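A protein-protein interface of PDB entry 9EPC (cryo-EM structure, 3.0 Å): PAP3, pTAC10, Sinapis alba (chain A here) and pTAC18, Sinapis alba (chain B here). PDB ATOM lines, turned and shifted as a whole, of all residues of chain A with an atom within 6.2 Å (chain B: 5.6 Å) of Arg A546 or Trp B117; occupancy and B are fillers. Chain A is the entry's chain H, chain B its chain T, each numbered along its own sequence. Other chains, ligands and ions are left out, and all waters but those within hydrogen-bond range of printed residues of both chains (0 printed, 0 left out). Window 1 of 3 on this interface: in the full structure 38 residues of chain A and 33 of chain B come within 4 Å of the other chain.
NE1 of Trp B117 sits at hydrogen-bond distance from O of Leu A541 (3.2 Å). OE1 of Glu B119 is in salt-bridge range of NH2 of Arg A385 (2.7 Å). The guanidinium group (NH1) of Arg A546 is in salt-bridge range of the side-chain carboxylate (OE1) of Glu B119. NE of Arg A534 lies close to NZ of Lys B116 (2.9 Å).
The backbone carbonyl oxygen (O) of Trp B80 lies within hydrogen-bond range of the backbone NH (N) of Trp B117, 2.6 Å away. The side-chain hydroxyl (OH) of Tyr A547 sits at hydrogen-bond distance from the guanidinium group (NH2) of Arg A385 (3.1 Å). The backbone NH of Lys A548 lies within hydrogen-bond range of the backbone carbonyl oxygen of Arg A385 (3.3 Å). The backbone carbonyl oxygen (O) of Pro A540 sits close to the guanidinium group (NH1) of Arg A534 (3.4 Å). The side-chain carboxylate (OE1) of Glu A543 is in salt-bridge range of the guanidinium group (NE) of Arg A546, at 3.1 Å.
Among the printed residues, merely in contact across the chains: Glu A542 with Trp B117, Glu A543 with Trp B117, Arg A546 with Trp B117, Pro A540 with Trp B117, Pro A544 with Trp B117 and Leu A541 with Lys B116.
Printed residues of chain B within 4 Å of Arg A546: Trp B117 and Glu B119. Trp B117 touches six residues of chain A. Of the printed residues of chain B, Glu A543 touches Trp B117. Of the printed residues of chain B, Leu A541 touches Lys B116 (3.9 Å) and Trp B117 (3.2 Å). Of the printed residues of chain B, Arg A534 touches Lys B116 (2.9 Å). Printed residues of chain A within 4 Å of Glu B119: Arg A385 (2.7 Å) and Arg A546 (3.1 Å). Leu B118 touches none of the printed residues of chain A. The nearest residue of chain A that does not touch Trp B117 is Arg A534 (4.1 Å). The nearest printed residue of chain A that does not touch Glu B119 is Tyr A547 (4.3 Å).
Of the 15 printed residues of chain A, 8 touch a printed residue of chain B. Hydrophobic or aromatic side chains of chain A that line the printed part of chain B: Pro A544. Printed residues of chain B that touch a printed residue of chain A: Lys B116, Trp B117 and Glu B119. Hydrophobic or aromatic side chains of chain B within 4 Å of the printed part of chain A: Trp B117. Among the printed residues, 10 pairs touch across the chains.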
ATOM      1  N   ARG A 376     -28.583 -31.419  21.539  1.00  0.00           N
ATOM      2  CA  ARG A 376     -29.335 -30.461  22.338  1.00  0.00           C
ATOM      3  C   ARG A 376     -30.597 -31.080  22.919  1.00  0.00           C
ATOM      4  O   ARG A 376     -31.042 -30.672  23.997  1.00  0.00           O
ATOM      5  CB  ARG A 376     -29.678 -29.235  21.493  1.00  0.00           C
ATOM      6  CG  ARG A 376     -29.679 -27.932  22.264  1.00  0.00           C
ATOM      7  CD  ARG A 376     -29.795 -26.745  21.325  1.00  0.00           C
ATOM      8  NE  ARG A 376     -28.593 -26.551  20.523  1.00  0.00           N
ATOM      9  CZ  ARG A 376     -27.633 -25.686  20.816  1.00  0.00           C
ATOM     10  NH1 ARG A 376     -27.691 -24.928  21.898  1.00  0.00           N
ATOM     11  NH2 ARG A 376     -26.591 -25.573  19.999  1.00  0.00           N
ATOM     12  N   PRO A 382     -21.717 -30.166  22.812  1.00  0.00           N
ATOM     13  CA  PRO A 382     -21.674 -29.838  21.384  1.00  0.00           C
ATOM     14  C   PRO A 382     -20.454 -30.446  20.710  1.00  0.00           C
ATOM     15  O   PRO A 382     -19.516 -30.923  21.352  1.00  0.00           O
ATOM     16  CB  PRO A 382     -21.610 -28.309  21.373  1.00  0.00           C
ATOM     17  CG  PRO A 382     -21.015 -27.953  22.689  1.00  0.00           C
ATOM     18  CD  PRO A 382     -21.535 -28.974  23.657  1.00  0.00           C
ATOM     19  N   GLU A 383     -20.486 -30.428  19.387  1.00  0.00           N
ATOM     20  CA  GLU A 383     -19.373 -30.950  18.607  1.00  0.00           C
ATOM     21  C   GLU A 383     -18.184 -30.008  18.724  1.00  0.00           C
ATOM     22  O   GLU A 383     -18.301 -28.830  18.365  1.00  0.00           O
ATOM     23  CB  GLU A 383     -19.779 -31.118  17.148  1.00  0.00           C
ATOM     24  CG  GLU A 383     -18.715 -31.765  16.278  1.00  0.00           C
ATOM     25  CD  GLU A 383     -18.507 -33.233  16.599  1.00  0.00           C
ATOM     26  OE1 GLU A 383     -19.397 -33.842  17.228  1.00  0.00           O
ATOM     27  OE2 GLU A 383     -17.450 -33.779  16.220  1.00  0.00           O
ATOM     28  N   PRO A 384     -17.037 -30.470  19.213  1.00  0.00           N
ATOM     29  CA  PRO A 384     -15.893 -29.569  19.376  1.00  0.00           C
ATOM     30  C   PRO A 384     -15.356 -29.095  18.037  1.00  0.00           C
ATOM     31  O   PRO A 384     -15.450 -29.785  17.019  1.00  0.00           O
ATOM     32  CB  PRO A 384     -14.865 -30.434  20.112  1.00  0.00           C
ATOM     33  CG  PRO A 384     -15.219 -31.828  19.727  1.00  0.00           C
ATOM     34  CD  PRO A 384     -16.716 -31.850  19.606  1.00  0.00           C
ATOM     35  N   ARG A 385     -14.790 -27.893  18.049  1.00  0.00           N
ATOM     36  CA  ARG A 385     -14.163 -27.309  16.876  1.00  0.00           C
ATOM     37  C   ARG A 385     -12.814 -26.731  17.269  1.00  0.00           C
ATOM     38  O   ARG A 385     -12.572 -26.400  18.432  1.00  0.00           O
ATOM     39  CB  ARG A 385     -15.038 -26.221  16.240  1.00  0.00           C
ATOM     40  CG  ARG A 385     -16.389 -26.715  15.755  1.00  0.00           C
ATOM     41  CD  ARG A 385     -17.023 -25.732  14.786  1.00  0.00           C
ATOM     42  NE  ARG A 385     -17.245 -24.424  15.388  1.00  0.00           N
ATOM     43  CZ  ARG A 385     -18.379 -24.046  15.960  1.00  0.00           C
ATOM     44  NH1 ARG A 385     -19.421 -24.857  16.033  1.00  0.00           N
ATOM     45  NH2 ARG A 385     -18.471 -22.821  16.470  1.00  0.00           N
ATOM     46  N   ARG A 534     -18.538 -12.662  33.732  1.00  0.00           N
ATOM     47  CA  ARG A 534     -18.180 -14.074  33.681  1.00  0.00           C
ATOM     48  C   ARG A 534     -16.751 -14.297  34.158  1.00  0.00           C
ATOM     49  O   ARG A 534     -16.466 -15.291  34.834  1.00  0.00           O
ATOM     50  CB  ARG A 534     -18.372 -14.606  32.264  1.00  0.00           C
ATOM     51  CG  ARG A 534     -19.805 -14.512  31.785  1.00  0.00           C
ATOM     52  CD  ARG A 534     -19.967 -15.054  30.384  1.00  0.00           C
ATOM     53  NE  ARG A 534     -21.369 -15.072  29.989  1.00  0.00           N
ATOM     54  CZ  ARG A 534     -22.199 -16.073  30.237  1.00  0.00           C
ATOM     55  NH1 ARG A 534     -21.797 -17.163  30.868  1.00  0.00           N
ATOM     56  NH2 ARG A 534     -23.465 -15.979  29.841  1.00  0.00           N
ATOM     57  N   PRO A 540     -17.923 -19.404  31.972  1.00  0.00           N
ATOM     58  CA  PRO A 540     -17.193 -19.508  30.704  1.00  0.00           C
ATOM     59  C   PRO A 540     -17.543 -18.371  29.759  1.00  0.00           C
ATOM     60  O   PRO A 540     -18.708 -17.993  29.614  1.00  0.00           O
ATOM     61  CB  PRO A 540     -17.651 -20.859  30.145  1.00  0.00           C
ATOM     62  CG  PRO A 540     -18.988 -21.081  30.768  1.00  0.00           C
ATOM     63  CD  PRO A 540     -18.895 -20.497  32.144  1.00  0.00           C
ATOM     64  N   LEU A 541     -16.514 -17.825  29.110  1.00  0.00           N
ATOM     65  CA  LEU A 541     -16.740 -16.766  28.133  1.00  0.00           C
ATOM     66  C   LEU A 541     -17.378 -17.315  26.865  1.00  0.00           C
ATOM     67  O   LEU A 541     -18.297 -16.703  26.310  1.00  0.00           O
ATOM     68  CB  LEU A 541     -15.425 -16.061  27.809  1.00  0.00           C
ATOM     69  CG  LEU A 541     -14.724 -15.401  28.994  1.00  0.00           C
ATOM     70  CD1 LEU A 541     -13.446 -14.715  28.544  1.00  0.00           C
ATOM     71  CD2 LEU A 541     -15.654 -14.414  29.678  1.00  0.00           C
ATOM     72  N   GLU A 542     -16.905 -18.460  26.394  1.00  0.00           N
ATOM     73  CA  GLU A 542     -17.454 -19.131  25.227  1.00  0.00           C
ATOM     74  C   GLU A 542     -18.242 -20.356  25.671  1.00  0.00           C
ATOM     75  O   GLU A 542     -18.321 -20.681  26.860  1.00  0.00           O
ATOM     76  CB  GLU A 542     -16.343 -19.515  24.248  1.00  0.00           C
ATOM     77  CG  GLU A 542     -15.472 -20.670  24.713  1.00  0.00           C
ATOM     78  CD  GLU A 542     -14.541 -20.288  25.848  1.00  0.00           C
ATOM     79  OE1 GLU A 542     -14.368 -19.077  26.096  1.00  0.00           O
ATOM     80  OE2 GLU A 542     -13.985 -21.200  26.495  1.00  0.00           O
ATOM     81  N   GLU A 543     -18.827 -21.041  24.702  1.00  0.00           N
ATOM     82  CA  GLU A 543     -19.630 -22.214  25.006  1.00  0.00           C
ATOM     83  C   GLU A 543     -18.734 -23.341  25.507  1.00  0.00           C
ATOM     84  O   GLU A 543     -17.745 -23.679  24.846  1.00  0.00           O
ATOM     85  CB  GLU A 543     -20.405 -22.660  23.770  1.00  0.00           C
ATOM     86  CG  GLU A 543     -21.416 -23.756  24.034  1.00  0.00           C
ATOM     87  CD  GLU A 543     -22.202 -24.129  22.795  1.00  0.00           C
ATOM     88  OE1 GLU A 543     -21.797 -23.718  21.688  1.00  0.00           O
ATOM     89  OE2 GLU A 543     -23.227 -24.828  22.927  1.00  0.00           O
ATOM     90  N   PRO A 544     -19.029 -23.931  26.663  1.00  0.00           N
ATOM     91  CA  PRO A 544     -18.228 -25.064  27.138  1.00  0.00           C
ATOM     92  C   PRO A 544     -18.330 -26.244  26.186  1.00  0.00           C
ATOM     93  O   PRO A 544     -19.344 -26.445  25.515  1.00  0.00           O
ATOM     94  CB  PRO A 544     -18.843 -25.390  28.503  1.00  0.00           C
ATOM     95  CG  PRO A 544     -19.547 -24.141  28.912  1.00  0.00           C
ATOM     96  CD  PRO A 544     -20.046 -23.524  27.644  1.00  0.00           C
ATOM     97  N   GLY A 545     -17.262 -27.024  26.128  1.00  0.00           N
ATOM     98  CA  GLY A 545     -17.202 -28.136  25.184  1.00  0.00           C
ATOM     99  C   GLY A 545     -16.811 -27.716  23.790  1.00  0.00           C
ATOM    100  O   GLY A 545     -15.878 -28.280  23.211  1.00  0.00           O
ATOM    101  N   ARG A 546     -17.506 -26.733  23.231  1.00  0.00           N
ATOM    102  CA  ARG A 546     -17.114 -26.176  21.947  1.00  0.00           C
ATOM    103  C   ARG A 546     -15.780 -25.449  22.079  1.00  0.00           C
ATOM    104  O   ARG A 546     -15.417 -24.966  23.154  1.00  0.00           O
ATOM    105  CB  ARG A 546     -18.193 -25.222  21.435  1.00  0.00           C
ATOM    106  CG  ARG A 546     -18.035 -24.808  19.985  1.00  0.00           C
ATOM    107  CD  ARG A 546     -19.158 -23.882  19.558  1.00  0.00           C
ATOM    108  NE  ARG A 546     -19.226 -22.690  20.394  1.00  0.00           N
ATOM    109  CZ  ARG A 546     -20.064 -21.683  20.195  1.00  0.00           C
ATOM    110  NH1 ARG A 546     -20.924 -21.687  19.189  1.00  0.00           N
ATOM    111  NH2 ARG A 546     -20.039 -20.644  21.025  1.00  0.00           N
ATOM    112  N   TYR A 547     -15.042 -25.393  20.970  1.00  0.00           N
ATOM    113  CA  TYR A 547     -13.723 -24.763  20.915  1.00  0.00           C
ATOM    114  C   TYR A 547     -12.750 -25.438  21.882  1.00  0.00           C
ATOM    115  O   TYR A 547     -12.196 -24.820  22.792  1.00  0.00           O
ATOM    116  CB  TYR A 547     -13.817 -23.257  21.189  1.00  0.00           C
ATOM    117  CG  TYR A 547     -14.600 -22.495  20.150  1.00  0.00           C
ATOM    118  CD1 TYR A 547     -14.756 -22.994  18.865  1.00  0.00           C
ATOM    119  CD2 TYR A 547     -15.183 -21.272  20.453  1.00  0.00           C
ATOM    120  CE1 TYR A 547     -15.471 -22.300  17.913  1.00  0.00           C
ATOM    121  CE2 TYR A 547     -15.901 -20.571  19.508  1.00  0.00           C
ATOM    122  CZ  TYR A 547     -16.042 -21.090  18.238  1.00  0.00           C
ATOM    123  OH  TYR A 547     -16.756 -20.394  17.290  1.00  0.00           O
ATOM    124  N   LYS A 548     -12.554 -26.736  21.667  1.00  0.00           N
ATOM    125  CA  LYS A 548     -11.575 -27.476  22.444  1.00  0.00           C
ATOM    126  C   LYS A 548     -10.161 -27.067  22.037  1.00  0.00           C
ATOM    127  O   LYS A 548      -9.938 -26.612  20.912  1.00  0.00           O
ATOM    128  CB  LYS A 548     -11.763 -28.978  22.256  1.00  0.00           C
ATOM    129  CG  LYS A 548     -12.584 -29.626  23.354  1.00  0.00           C
ATOM    130  CD  LYS A 548     -12.664 -31.129  23.177  1.00  0.00           C
ATOM    131  CE  LYS A 548     -13.328 -31.783  24.374  1.00  0.00           C
ATOM    132  NZ  LYS A 548     -14.672 -31.204  24.646  1.00  0.00           N
ATOM    133  N   TRP B  80     -24.768 -15.249  18.214  1.00  0.00           N
ATOM    134  CA  TRP B  80     -24.973 -14.340  19.339  1.00  0.00           C
ATOM    135  C   TRP B  80     -23.865 -14.546  20.360  1.00  0.00           C
ATOM    136  O   TRP B  80     -23.885 -15.501  21.138  1.00  0.00           O
ATOM    137  CB  TRP B  80     -26.346 -14.562  19.960  1.00  0.00           C
ATOM    138  CG  TRP B  80     -27.452 -13.958  19.162  1.00  0.00           C
ATOM    139  CD1 TRP B  80     -28.046 -12.751  19.374  1.00  0.00           C
ATOM    140  CD2 TRP B  80     -28.093 -14.525  18.016  1.00  0.00           C
ATOM    141  NE1 TRP B  80     -29.022 -12.533  18.434  1.00  0.00           N
ATOM    142  CE2 TRP B  80     -29.069 -13.608  17.587  1.00  0.00           C
ATOM    143  CE3 TRP B  80     -27.937 -15.721  17.312  1.00  0.00           C
ATOM    144  CZ2 TRP B  80     -29.885 -13.849  16.487  1.00  0.00           C
ATOM    145  CZ3 TRP B  80     -28.748 -15.958  16.221  1.00  0.00           C
ATOM    146  CH2 TRP B  80     -29.710 -15.028  15.819  1.00  0.00           C
ATOM    147  N   GLN B  81     -22.886 -13.639  20.359  1.00  0.00           N
ATOM    148  CA  GLN B  81     -21.860 -13.630  21.393  1.00  0.00           C
ATOM    149  C   GLN B  81     -22.375 -13.088  22.717  1.00  0.00           C
ATOM    150  O   GLN B  81     -21.659 -13.170  23.720  1.00  0.00           O
ATOM    151  CB  GLN B  81     -20.657 -12.806  20.934  1.00  0.00           C
ATOM    152  CG  GLN B  81     -19.863 -13.434  19.803  1.00  0.00           C
ATOM    153  CD  GLN B  81     -18.948 -12.438  19.120  1.00  0.00           C
ATOM    154  OE1 GLN B  81     -18.941 -11.255  19.456  1.00  0.00           O
ATOM    155  NE2 GLN B  81     -18.174 -12.913  18.152  1.00  0.00           N
ATOM    156  N   VAL B  82     -23.583 -12.529  22.740  1.00  0.00           N
ATOM    157  CA  VAL B  82     -24.192 -12.026  23.965  1.00  0.00           C
ATOM    158  C   VAL B  82     -25.701 -12.145  23.816  1.00  0.00           C
ATOM    159  O   VAL B  82     -26.233 -12.147  22.702  1.00  0.00           O
ATOM    160  CB  VAL B  82     -23.758 -10.569  24.261  1.00  0.00           C
ATOM    161  CG1 VAL B  82     -24.410  -9.608  23.288  1.00  0.00           C
ATOM    162  CG2 VAL B  82     -24.075 -10.191  25.699  1.00  0.00           C
ATOM    163  N   PRO B 115     -30.554 -16.555  22.869  1.00  0.00           N
ATOM    164  CA  PRO B 115     -29.521 -16.771  23.884  1.00  0.00           C
ATOM    165  C   PRO B 115     -28.125 -16.643  23.290  1.00  0.00           C
ATOM    166  O   PRO B 115     -27.937 -16.493  22.083  1.00  0.00           O
ATOM    167  CB  PRO B 115     -29.792 -18.200  24.357  1.00  0.00           C
ATOM    168  CG  PRO B 115     -30.387 -18.863  23.165  1.00  0.00           C
ATOM    169  CD  PRO B 115     -31.213 -17.811  22.475  1.00  0.00           C
ATOM    170  N   LYS B 116     -27.136 -16.707  24.175  1.00  0.00           N
ATOM    171  CA  LYS B 116     -25.749 -16.633  23.749  1.00  0.00           C
ATOM    172  C   LYS B 116     -25.344 -17.903  23.009  1.00  0.00           C
ATOM    173  O   LYS B 116     -25.991 -18.949  23.108  1.00  0.00           O
ATOM    174  CB  LYS B 116     -24.825 -16.425  24.947  1.00  0.00           C
ATOM    175  CG  LYS B 116     -25.054 -15.129  25.694  1.00  0.00           C
ATOM    176  CD  LYS B 116     -23.972 -14.906  26.735  1.00  0.00           C
ATOM    177  CE  LYS B 116     -22.591 -15.027  26.117  1.00  0.00           C
ATOM    178  NZ  LYS B 116     -21.511 -14.695  27.082  1.00  0.00           N
ATOM    179  N   TRP B 117     -24.257 -17.791  22.248  1.00  0.00           N
ATOM    180  CA  TRP B 117     -23.624 -18.919  21.571  1.00  0.00           C
ATOM    181  C   TRP B 117     -24.568 -19.621  20.602  1.00  0.00           C
ATOM    182  O   TRP B 117     -24.398 -20.810  20.317  1.00  0.00           O
ATOM    183  CB  TRP B 117     -23.070 -19.923  22.587  1.00  0.00           C
ATOM    184  CG  TRP B 117     -22.247 -19.282  23.655  1.00  0.00           C
ATOM    185  CD1 TRP B 117     -21.423 -18.205  23.517  1.00  0.00           C
ATOM    186  CD2 TRP B 117     -22.183 -19.664  25.031  1.00  0.00           C
ATOM    187  NE1 TRP B 117     -20.841 -17.898  24.721  1.00  0.00           N
ATOM    188  CE2 TRP B 117     -21.293 -18.780  25.668  1.00  0.00           C
ATOM    189  CE3 TRP B 117     -22.788 -20.670  25.786  1.00  0.00           C
ATOM    190  CZ2 TRP B 117     -20.994 -18.871  27.023  1.00  0.00           C
ATOM    191  CZ3 TRP B 117     -22.491 -20.760  27.131  1.00  0.00           C
ATOM    192  CH2 TRP B 117     -21.601 -19.866  27.736  1.00  0.00           C
ATOM    193  N   LEU B 118     -25.565 -18.906  20.090  1.00  0.00           N
ATOM    194  CA  LEU B 118     -26.509 -19.464  19.133  1.00  0.00           C
ATOM    195  C   LEU B 118     -26.037 -19.147  17.721  1.00  0.00           C
ATOM    196  O   LEU B 118     -25.910 -17.977  17.352  1.00  0.00           O
ATOM    197  CB  LEU B 118     -27.910 -18.903  19.367  1.00  0.00           C
ATOM    198  CG  LEU B 118     -28.921 -19.127  18.241  1.00  0.00           C
ATOM    199  CD1 LEU B 118     -29.164 -20.607  18.020  1.00  0.00           C
ATOM    200  CD2 LEU B 118     -30.224 -18.409  18.545  1.00  0.00           C
ATOM    201  N   GLU B 119     -25.778 -20.186  16.934  1.00  0.00           N
ATOM    202  CA  GLU B 119     -25.387 -20.030  15.541  1.00  0.00           C
ATOM    203  C   GLU B 119     -26.597 -20.309  14.661  1.00  0.00           C
ATOM    204  O   GLU B 119     -27.132 -21.423  14.667  1.00  0.00           O
ATOM    205  CB  GLU B 119     -24.233 -20.967  15.188  1.00  0.00           C
ATOM    206  CG  GLU B 119     -22.934 -20.618  15.882  1.00  0.00           C
ATOM    207  CD  GLU B 119     -21.794 -21.520  15.466  1.00  0.00           C
ATOM    208  OE1 GLU B 119     -20.712 -21.435  16.082  1.00  0.00           O
ATOM    209  OE2 GLU B 119     -21.979 -22.314  14.521  1.00  0.00           O
